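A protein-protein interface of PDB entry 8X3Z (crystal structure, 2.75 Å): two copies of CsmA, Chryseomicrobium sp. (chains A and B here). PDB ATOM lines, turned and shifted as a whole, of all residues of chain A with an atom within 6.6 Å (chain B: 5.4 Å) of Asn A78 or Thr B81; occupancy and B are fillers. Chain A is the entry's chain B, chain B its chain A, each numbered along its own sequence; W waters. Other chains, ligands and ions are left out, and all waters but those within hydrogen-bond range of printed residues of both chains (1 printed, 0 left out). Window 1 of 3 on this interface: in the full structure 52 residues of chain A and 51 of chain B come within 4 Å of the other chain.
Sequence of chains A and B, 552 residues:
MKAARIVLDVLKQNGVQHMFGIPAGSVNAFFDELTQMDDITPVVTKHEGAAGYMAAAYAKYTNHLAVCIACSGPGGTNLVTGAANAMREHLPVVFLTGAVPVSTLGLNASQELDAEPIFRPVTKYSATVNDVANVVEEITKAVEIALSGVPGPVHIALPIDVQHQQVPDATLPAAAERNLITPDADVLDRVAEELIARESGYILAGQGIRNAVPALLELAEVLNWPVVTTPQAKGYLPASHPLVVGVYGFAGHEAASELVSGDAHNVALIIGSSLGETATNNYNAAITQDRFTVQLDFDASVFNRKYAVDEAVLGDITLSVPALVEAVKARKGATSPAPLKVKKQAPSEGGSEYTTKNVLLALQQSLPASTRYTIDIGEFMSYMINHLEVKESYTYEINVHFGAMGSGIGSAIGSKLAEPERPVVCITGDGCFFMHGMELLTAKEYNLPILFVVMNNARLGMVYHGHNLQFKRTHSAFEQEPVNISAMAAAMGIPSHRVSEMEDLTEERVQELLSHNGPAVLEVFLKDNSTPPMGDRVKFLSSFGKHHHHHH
The side-chain hydroxyl (OG1) of Thr A81 is in hydrogen-bond range of the side-chain hydroxyl (OG1) of Thr B77 (2.7 Å).
The side-chain hydroxyl (OG1) of Thr A81 is in hydrogen-bond range of the side-chain amide oxygen (OD1) of Asn B78 (2.4 Å).
The side-chain hydroxyl of Thr B81 is in hydrogen-bond range of the side-chain amide oxygen of Asn A78, at 2.5 Å.
OG1 of Thr B81 is in hydrogen-bond range of OG1 of Thr A77.
The side-chain amide nitrogen of Asn A78 lies within hydrogen-bond range of the side-chain carboxylate of Glu A48 (3.1 Å).
The backbone carbonyl oxygen (O) of Gly A73 sits at hydrogen-bond distance from the side-chain hydroxyl (OG1) of Thr A77 (3.3 Å).
ND1 of His A47 sits at hydrogen-bond distance from N of Gly A49, at 2.9 Å.
OG1 of Thr A77 sits at hydrogen-bond distance from O of Pro A74 (3.2 Å).
Among the printed residues, pairs that only touch across the chains: Pro A74 with Phe B402 (3.3 Å), His A47 with Met B435 (3.5 Å), Pro A74 with Ala B404 (3.6 Å), Glu A48 with Met B435 (3.7 Å), His A47 with His B436 (3.7 Å), Gly A73 with Phe B402 (3.7 Å), Val A80 with Thr B77 (3.9 Å) and Thr A77 with Phe B402 (3.98 Å).
Of chain B, only Thr B81 comes within 4 Å of Asn A78.
Printed residues of chain A within 4 Å of Thr B81: Thr A77 and Asn A78.
Of the printed residues of chain B, Thr A81 touches Thr B77 (2.7 Å) and Asn B78 (2.4 Å).
Of the printed residues of chain A, Asn B78 touches Thr A81.
Gly A76 touches none of the printed residues of chain B.
Gly A82 touches none of the printed residues of chain B.
The nearest printed residue of chain B that does not touch Gly A73 is Thr B81 (5.8 Å).
Hydrophobic or aromatic side chains of chain A within 4 Å of the printed part of chain B: His A47, Pro A74 and Val A80.
Of the 15 printed residues of chain B, 7 touch a printed residue of chain A.
Printed residues of chain B that touch a printed residue of chain A: Thr B77, Asn B78, Thr B81, Phe B402, Ala B404, Met B435 and His B436.
Hydrophobic or aromatic side chains of chain B within 4 Å of the printed part of chain A: Phe B402, Ala B404, Met B435 and His B436.
Among the printed residues, 12 pairs touch across the chains.
Among the printed residues, no Asp or Glu carboxylate lies within 4 Å of a Lys or Arg side-chain nitrogen of the other chain.
Thr A77 touches Thr B81, and with the chains exchanged Thr A81 touches Thr B77.
Asn A78 touches Thr B81, and with the chains exchanged Thr A81 touches Asn B78.
Val A80 touches Thr B77, but with the chains exchanged Thr A77 does not touch Val B80 (4.01 Å).
Positions printed for both chains: 77, 78, 79, 80, 81 and 82.
Of the 12 pairs that touch across the chains among the printed residues, 4 have their exchanged pair printed and touching as well.
Water W1 lies within hydrogen-bond range of the backbone carbonyl oxygen of Asn A78 (2.5 Å) and the side-chain amide oxygen of Asn B78 (3.2 Å).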
ATOM      1  N   HIS A  47      -5.054 -19.768  -2.472  1.00  0.00           N
ATOM      2  CA  HIS A  47      -6.290 -19.712  -3.250  1.00  0.00           C
ATOM      3  C   HIS A  47      -6.092 -18.652  -4.338  1.00  0.00           C
ATOM      4  O   HIS A  47      -5.532 -17.585  -4.059  1.00  0.00           O
ATOM      5  CB  HIS A  47      -7.481 -19.361  -2.335  1.00  0.00           C
ATOM      6  CG  HIS A  47      -8.825 -19.523  -2.968  1.00  0.00           C
ATOM      7  ND1 HIS A  47      -9.308 -18.666  -3.939  1.00  0.00           N
ATOM      8  CD2 HIS A  47      -9.804 -20.435  -2.750  1.00  0.00           C
ATOM      9  CE1 HIS A  47     -10.519 -19.056  -4.305  1.00  0.00           C
ATOM     10  NE2 HIS A  47     -10.846 -20.126  -3.598  1.00  0.00           N
ATOM     11  N   GLU A  48      -6.506 -18.934  -5.582  1.00  0.00           N
ATOM     12  CA  GLU A  48      -6.254 -17.949  -6.647  1.00  0.00           C
ATOM     13  C   GLU A  48      -7.071 -16.677  -6.466  1.00  0.00           C
ATOM     14  O   GLU A  48      -6.678 -15.617  -6.979  1.00  0.00           O
ATOM     15  CB  GLU A  48      -6.527 -18.524  -8.038  1.00  0.00           C
ATOM     16  CG  GLU A  48      -5.661 -19.747  -8.350  1.00  0.00           C
ATOM     17  CD  GLU A  48      -6.354 -21.079  -7.985  1.00  0.00           C
ATOM     18  OE1 GLU A  48      -6.052 -22.093  -8.638  1.00  0.00           O
ATOM     19  OE2 GLU A  48      -7.197 -21.118  -7.054  1.00  0.00           O
ATOM     20  N   GLY A  49      -8.201 -16.753  -5.760  1.00  0.00           N
ATOM     21  CA  GLY A  49      -8.913 -15.531  -5.446  1.00  0.00           C
ATOM     22  C   GLY A  49      -8.014 -14.522  -4.757  1.00  0.00           C
ATOM     23  O   GLY A  49      -7.952 -13.355  -5.146  1.00  0.00           O
ATOM     24  N   ALA A  50      -7.258 -14.969  -3.748  1.00  0.00           N
ATOM     25  CA  ALA A  50      -6.357 -14.032  -3.085  1.00  0.00           C
ATOM     26  C   ALA A  50      -5.243 -13.582  -4.018  1.00  0.00           C
ATOM     27  O   ALA A  50      -4.746 -12.467  -3.877  1.00  0.00           O
ATOM     28  CB  ALA A  50      -5.777 -14.633  -1.795  1.00  0.00           C
ATOM     29  N   ALA A  70      -3.427 -18.913 -13.462  1.00  0.00           N
ATOM     30  CA  ALA A  70      -4.166 -20.009 -12.850  1.00  0.00           C
ATOM     31  C   ALA A  70      -4.372 -21.108 -13.881  1.00  0.00           C
ATOM     32  O   ALA A  70      -4.331 -20.858 -15.096  1.00  0.00           O
ATOM     33  CB  ALA A  70      -5.527 -19.572 -12.272  1.00  0.00           C
ATOM     34  N   GLY A  73      -9.872 -24.229 -15.990  1.00  0.00           N
ATOM     35  CA  GLY A  73     -10.979 -24.637 -15.162  1.00  0.00           C
ATOM     36  C   GLY A  73     -11.051 -23.945 -13.813  1.00  0.00           C
ATOM     37  O   GLY A  73     -11.248 -22.727 -13.730  1.00  0.00           O
ATOM     38  N   PRO A  74     -10.911 -24.715 -12.725  1.00  0.00           N
ATOM     39  CA  PRO A  74     -11.152 -24.137 -11.386  1.00  0.00           C
ATOM     40  C   PRO A  74     -10.196 -23.007 -11.023  1.00  0.00           C
ATOM     41  O   PRO A  74     -10.627 -22.016 -10.419  1.00  0.00           O
ATOM     42  CB  PRO A  74     -11.021 -25.347 -10.442  1.00  0.00           C
ATOM     43  CG  PRO A  74     -10.452 -26.468 -11.263  1.00  0.00           C
ATOM     44  CD  PRO A  74     -10.780 -26.180 -12.687  1.00  0.00           C
ATOM     45  N   GLY A  75      -8.914 -23.104 -11.384  1.00  0.00           N
ATOM     46  CA  GLY A  75      -8.034 -21.958 -11.192  1.00  0.00           C
ATOM     47  C   GLY A  75      -8.549 -20.704 -11.885  1.00  0.00           C
ATOM     48  O   GLY A  75      -8.681 -19.646 -11.266  1.00  0.00           O
ATOM     49  N   GLY A  76      -8.877 -20.819 -13.177  1.00  0.00           N
ATOM     50  CA  GLY A  76      -9.392 -19.673 -13.913  1.00  0.00           C
ATOM     51  C   GLY A  76     -10.646 -19.088 -13.290  1.00  0.00           C
ATOM     52  O   GLY A  76     -10.759 -17.870 -13.129  1.00  0.00           O
ATOM     53  N   THR A  77     -11.608 -19.945 -12.917  1.00  0.00           N
ATOM     54  CA  THR A  77     -12.840 -19.398 -12.356  1.00  0.00           C
ATOM     55  C   THR A  77     -12.605 -18.802 -10.970  1.00  0.00           C
ATOM     56  O   THR A  77     -13.323 -17.872 -10.573  1.00  0.00           O
ATOM     57  CB  THR A  77     -13.974 -20.447 -12.306  1.00  0.00           C
ATOM     58  OG1 THR A  77     -13.550 -21.620 -11.614  1.00  0.00           O
ATOM     59  CG2 THR A  77     -14.496 -20.841 -13.694  1.00  0.00           C
ATOM     60  N   ASN A  78     -11.614 -19.309 -10.216  1.00  0.00           N
ATOM     61  CA  ASN A  78     -11.322 -18.708  -8.910  1.00  0.00           C
ATOM     62  C   ASN A  78     -10.794 -17.278  -9.020  1.00  0.00           C
ATOM     63  O   ASN A  78     -10.898 -16.518  -8.055  1.00  0.00           O
ATOM     64  CB  ASN A  78     -10.330 -19.567  -8.123  1.00  0.00           C
ATOM     65  CG  ASN A  78     -11.001 -20.737  -7.441  1.00  0.00           C
ATOM     66  OD1 ASN A  78     -12.219 -20.856  -7.492  1.00  0.00           O
ATOM     67  ND2 ASN A  78     -10.204 -21.636  -6.839  1.00  0.00           N
ATOM     68  N   LEU A  79     -10.240 -16.899 -10.173  1.00  0.00           N
ATOM     69  CA  LEU A  79      -9.730 -15.562 -10.413  1.00  0.00           C
ATOM     70  C   LEU A  79     -10.827 -14.571 -10.745  1.00  0.00           C
ATOM     71  O   LEU A  79     -10.569 -13.370 -10.724  1.00  0.00           O
ATOM     72  CB  LEU A  79      -8.744 -15.583 -11.577  1.00  0.00           C
ATOM     73  CG  LEU A  79      -7.434 -16.345 -11.467  1.00  0.00           C
ATOM     74  CD1 LEU A  79      -6.762 -16.340 -12.848  1.00  0.00           C
ATOM     75  CD2 LEU A  79      -6.514 -15.740 -10.372  1.00  0.00           C
ATOM     76  N   VAL A  80     -12.040 -15.030 -11.043  1.00  0.00           N
ATOM     77  CA  VAL A  80     -13.080 -14.103 -11.479  1.00  0.00           C
ATOM     78  C   VAL A  80     -13.345 -13.039 -10.416  1.00  0.00           C
ATOM     79  O   VAL A  80     -13.542 -11.865 -10.740  1.00  0.00           O
ATOM     80  CB  VAL A  80     -14.358 -14.872 -11.853  1.00  0.00           C
ATOM     81  CG1 VAL A  80     -15.501 -13.915 -12.083  1.00  0.00           C
ATOM     82  CG2 VAL A  80     -14.093 -15.642 -13.085  1.00  0.00           C
ATOM     83  N   THR A  81     -13.361 -13.417  -9.136  1.00  0.00           N
ATOM     84  CA  THR A  81     -13.544 -12.397  -8.111  1.00  0.00           C
ATOM     85  C   THR A  81     -12.433 -11.368  -8.189  1.00  0.00           C
ATOM     86  O   THR A  81     -12.683 -10.162  -8.108  1.00  0.00           O
ATOM     87  CB  THR A  81     -13.591 -13.004  -6.709  1.00  0.00           C
ATOM     88  OG1 THR A  81     -14.502 -14.103  -6.693  1.00  0.00           O
ATOM     89  CG2 THR A  81     -14.076 -11.944  -5.700  1.00  0.00           C
ATOM     90  N   GLY A  82     -11.187 -11.832  -8.332  1.00  0.00           N
ATOM     91  CA  GLY A  82     -10.058 -10.911  -8.349  1.00  0.00           C
ATOM     92  C   GLY A  82     -10.072  -9.948  -9.526  1.00  0.00           C
ATOM     93  O   GLY A  82      -9.585  -8.811  -9.415  1.00  0.00           O
ATOM     94  N   PHE A 119     -14.808 -14.257 -18.223  1.00  0.00           N
ATOM     95  CA  PHE A 119     -14.044 -13.047 -17.932  1.00  0.00           C
ATOM     96  C   PHE A 119     -14.561 -11.834 -18.704  1.00  0.00           C
ATOM     97  O   PHE A 119     -14.271 -10.696 -18.311  1.00  0.00           O
ATOM     98  CB  PHE A 119     -12.556 -13.275 -18.239  1.00  0.00           C
ATOM     99  CG  PHE A 119     -11.844 -14.087 -17.192  1.00  0.00           C
ATOM    100  CD1 PHE A 119     -11.269 -13.466 -16.089  1.00  0.00           C
ATOM    101  CD2 PHE A 119     -11.775 -15.474 -17.295  1.00  0.00           C
ATOM    102  CE1 PHE A 119     -10.631 -14.202 -15.121  1.00  0.00           C
ATOM    103  CE2 PHE A 119     -11.143 -16.238 -16.314  1.00  0.00           C
ATOM    104  CZ  PHE A 119     -10.565 -15.605 -15.232  1.00  0.00           C
ATOM    105  N   TYR B  53     -19.196 -26.469  -3.706  1.00  0.00           N
ATOM    106  CA  TYR B  53     -18.820 -27.887  -3.699  1.00  0.00           C
ATOM    107  C   TYR B  53     -19.737 -28.690  -2.780  1.00  0.00           C
ATOM    108  O   TYR B  53     -20.106 -29.828  -3.110  1.00  0.00           O
ATOM    109  CB  TYR B  53     -17.349 -28.080  -3.302  1.00  0.00           C
ATOM    110  CG  TYR B  53     -16.396 -27.231  -4.079  1.00  0.00           C
ATOM    111  CD1 TYR B  53     -16.625 -26.943  -5.420  1.00  0.00           C
ATOM    112  CD2 TYR B  53     -15.271 -26.681  -3.463  1.00  0.00           C
ATOM    113  CE1 TYR B  53     -15.748 -26.126  -6.131  1.00  0.00           C
ATOM    114  CE2 TYR B  53     -14.393 -25.862  -4.163  1.00  0.00           C
ATOM    115  CZ  TYR B  53     -14.630 -25.591  -5.492  1.00  0.00           C
ATOM    116  OH  TYR B  53     -13.734 -24.796  -6.165  1.00  0.00           O
ATOM    117  N   THR B  77     -19.322 -13.852  -7.461  1.00  0.00           N
ATOM    118  CA  THR B  77     -18.217 -14.345  -8.296  1.00  0.00           C
ATOM    119  C   THR B  77     -17.444 -15.477  -7.613  1.00  0.00           C
ATOM    120  O   THR B  77     -16.832 -16.311  -8.293  1.00  0.00           O
ATOM    121  CB  THR B  77     -17.229 -13.230  -8.664  1.00  0.00           C
ATOM    122  OG1 THR B  77     -16.652 -12.666  -7.472  1.00  0.00           O
ATOM    123  CG2 THR B  77     -17.883 -12.142  -9.496  1.00  0.00           C
ATOM    124  N   ASN B  78     -17.413 -15.503  -6.282  1.00  0.00           N
ATOM    125  CA  ASN B  78     -16.789 -16.641  -5.637  1.00  0.00           C
ATOM    126  C   ASN B  78     -17.556 -17.937  -5.912  1.00  0.00           C
ATOM    127  O   ASN B  78     -16.976 -19.023  -5.786  1.00  0.00           O
ATOM    128  CB  ASN B  78     -16.689 -16.397  -4.130  1.00  0.00           C
ATOM    129  CG  ASN B  78     -15.481 -15.560  -3.743  1.00  0.00           C
ATOM    130  OD1 ASN B  78     -14.646 -15.245  -4.583  1.00  0.00           O
ATOM    131  ND2 ASN B  78     -15.383 -15.200  -2.465  1.00  0.00           N
ATOM    132  N   LEU B  79     -18.847 -17.846  -6.267  1.00  0.00           N
ATOM    133  CA  LEU B  79     -19.684 -19.005  -6.558  1.00  0.00           C
ATOM    134  C   LEU B  79     -19.509 -19.532  -7.978  1.00  0.00           C
ATOM    135  O   LEU B  79     -19.981 -20.632  -8.276  1.00  0.00           O
ATOM    136  CB  LEU B  79     -21.170 -18.674  -6.319  1.00  0.00           C
ATOM    137  CG  LEU B  79     -21.765 -18.657  -4.908  1.00  0.00           C
ATOM    138  CD1 LEU B  79     -23.197 -18.140  -4.928  1.00  0.00           C
ATOM    139  CD2 LEU B  79     -21.707 -20.029  -4.219  1.00  0.00           C
ATOM    140  N   VAL B  80     -18.860 -18.776  -8.860  1.00  0.00           N
ATOM    141  CA  VAL B  80     -18.747 -19.189 -10.256  1.00  0.00           C
ATOM    142  C   VAL B  80     -18.009 -20.528 -10.386  1.00  0.00           C
ATOM    143  O   VAL B  80     -18.380 -21.370 -11.210  1.00  0.00           O
ATOM    144  CB  VAL B  80     -18.079 -18.071 -11.071  1.00  0.00           C
ATOM    145  CG1 VAL B  80     -17.571 -18.614 -12.403  1.00  0.00           C
ATOM    146  CG2 VAL B  80     -19.072 -16.963 -11.262  1.00  0.00           C
ATOM    147  N   THR B  81     -16.951 -20.748  -9.594  1.00  0.00           N
ATOM    148  CA  THR B  81     -16.261 -22.038  -9.648  1.00  0.00           C
ATOM    149  C   THR B  81     -17.218 -23.163  -9.309  1.00  0.00           C
ATOM    150  O   THR B  81     -17.317 -24.148 -10.045  1.00  0.00           O
ATOM    151  CB  THR B  81     -15.075 -22.052  -8.692  1.00  0.00           C
ATOM    152  OG1 THR B  81     -14.232 -20.945  -9.007  1.00  0.00           O
ATOM    153  CG2 THR B  81     -14.272 -23.338  -8.824  1.00  0.00           C
ATOM    154  N   GLY B  82     -17.993 -22.994  -8.232  1.00  0.00           N
ATOM    155  CA  GLY B  82     -18.925 -24.035  -7.823  1.00  0.00           C
ATOM    156  C   GLY B  82     -20.005 -24.318  -8.855  1.00  0.00           C
ATOM    157  O   GLY B  82     -20.462 -25.460  -8.987  1.00  0.00           O
ATOM    158  N   ALA B  83     -20.403 -23.297  -9.613  1.00  0.00           N
ATOM    159  CA  ALA B  83     -21.382 -23.464 -10.685  1.00  0.00           C
ATOM    160  C   ALA B  83     -20.773 -24.133 -11.906  1.00  0.00           C
ATOM    161  O   ALA B  83     -21.425 -24.974 -12.533  1.00  0.00           O
ATOM    162  CB  ALA B  83     -21.973 -22.110 -11.081  1.00  0.00           C
ATOM    163  N   ALA B  84     -19.549 -23.758 -12.289  1.00  0.00           N
ATOM    164  CA  ALA B  84     -18.891 -24.470 -13.378  1.00  0.00           C
ATOM    165  C   ALA B  84     -18.748 -25.956 -13.047  1.00  0.00           C
ATOM    166  O   ALA B  84     -18.977 -26.823 -13.908  1.00  0.00           O
ATOM    167  CB  ALA B  84     -17.529 -23.850 -13.684  1.00  0.00           C
ATOM    168  N   ASN B  85     -18.406 -26.274 -11.791  1.00  0.00           N
ATOM    169  CA  ASN B  85     -18.304 -27.673 -11.413  1.00  0.00           C
ATOM    170  C   ASN B  85     -19.654 -28.380 -11.531  1.00  0.00           C
ATOM    171  O   ASN B  85     -19.764 -29.444 -12.159  1.00  0.00           O
ATOM    172  CB  ASN B  85     -17.759 -27.799 -10.002  1.00  0.00           C
ATOM    173  CG  ASN B  85     -17.638 -29.266  -9.565  1.00  0.00           C
ATOM    174  OD1 ASN B  85     -16.939 -30.066 -10.203  1.00  0.00           O
ATOM    175  ND2 ASN B  85     -18.349 -29.627  -8.503  1.00  0.00           N
ATOM    176  N   ALA B  86     -20.695 -27.791 -10.933  1.00  0.00           N
ATOM    177  CA  ALA B  86     -22.034 -28.360 -10.997  1.00  0.00           C
ATOM    178  C   ALA B  86     -22.524 -28.486 -12.427  1.00  0.00           C
ATOM    179  O   ALA B  86     -23.278 -29.419 -12.742  1.00  0.00           O
ATOM    180  CB  ALA B  86     -23.009 -27.504 -10.191  1.00  0.00           C
ATOM    181  N   PHE B 402     -13.707 -31.549 -13.547  1.00  0.00           N
ATOM    182  CA  PHE B 402     -13.378 -30.185 -13.295  1.00  0.00           C
ATOM    183  C   PHE B 402     -12.231 -30.191 -12.346  1.00  0.00           C
ATOM    184  O   PHE B 402     -11.319 -29.481 -12.545  1.00  0.00           O
ATOM    185  CB  PHE B 402     -14.550 -29.476 -12.682  1.00  0.00           C
ATOM    186  CG  PHE B 402     -14.489 -27.988 -12.756  1.00  0.00           C
ATOM    187  CD1 PHE B 402     -14.435 -27.350 -13.946  1.00  0.00           C
ATOM    188  CD2 PHE B 402     -14.503 -27.248 -11.636  1.00  0.00           C
ATOM    189  CE1 PHE B 402     -14.393 -26.011 -14.011  1.00  0.00           C
ATOM    190  CE2 PHE B 402     -14.448 -25.909 -11.698  1.00  0.00           C
ATOM    191  CZ  PHE B 402     -14.412 -25.289 -12.885  1.00  0.00           C
ATOM    192  N   ALA B 404     -11.714 -29.224  -8.892  1.00  0.00           N
ATOM    193  CA  ALA B 404     -11.357 -28.074  -8.074  1.00  0.00           C
ATOM    194  C   ALA B 404     -10.744 -28.546  -6.757  1.00  0.00           C
ATOM    195  O   ALA B 404     -11.369 -29.323  -6.023  1.00  0.00           O
ATOM    196  CB  ALA B 404     -12.587 -27.205  -7.809  1.00  0.00           C
ATOM    197  N   MET B 435      -6.214 -24.237   0.784  1.00  0.00           N
ATOM    198  CA  MET B 435      -7.204 -23.570   0.019  1.00  0.00           C
ATOM    199  C   MET B 435      -8.536 -23.600   0.679  1.00  0.00           C
ATOM    200  O   MET B 435      -9.162 -22.609   0.820  1.00  0.00           O
ATOM    201  CB  MET B 435      -7.325 -24.221  -1.324  1.00  0.00           C
ATOM    202  CG  MET B 435      -7.894 -23.332  -2.392  1.00  0.00           C
ATOM    203  SD  MET B 435      -7.899 -24.023  -4.007  1.00  0.00           S
ATOM    204  CE  MET B 435      -6.303 -23.712  -4.599  1.00  0.00           C
ATOM    205  N   HIS B 436      -8.973 -24.753   1.099  1.00  0.00           N
ATOM    206  CA  HIS B 436     -10.262 -24.831   1.694  1.00  0.00           C
ATOM    207  C   HIS B 436     -10.403 -25.471   3.020  1.00  0.00           C
ATOM    208  O   HIS B 436     -11.464 -25.661   3.443  1.00  0.00           O
ATOM    209  CB  HIS B 436     -11.246 -25.432   0.722  1.00  0.00           C
ATOM    210  CG  HIS B 436     -11.668 -24.488  -0.340  1.00  0.00           C
ATOM    211  ND1 HIS B 436     -11.547 -24.758  -1.665  1.00  0.00           N
ATOM    212  CD2 HIS B 436     -12.179 -23.252  -0.256  1.00  0.00           C
ATOM    213  CE1 HIS B 436     -11.996 -23.743  -2.354  1.00  0.00           C
ATOM    214  NE2 HIS B 436     -12.372 -22.810  -1.523  1.00  0.00           N
HETATM  215  O   HOH W   1     -12.362 -17.010  -6.029  1.00  0.00           O
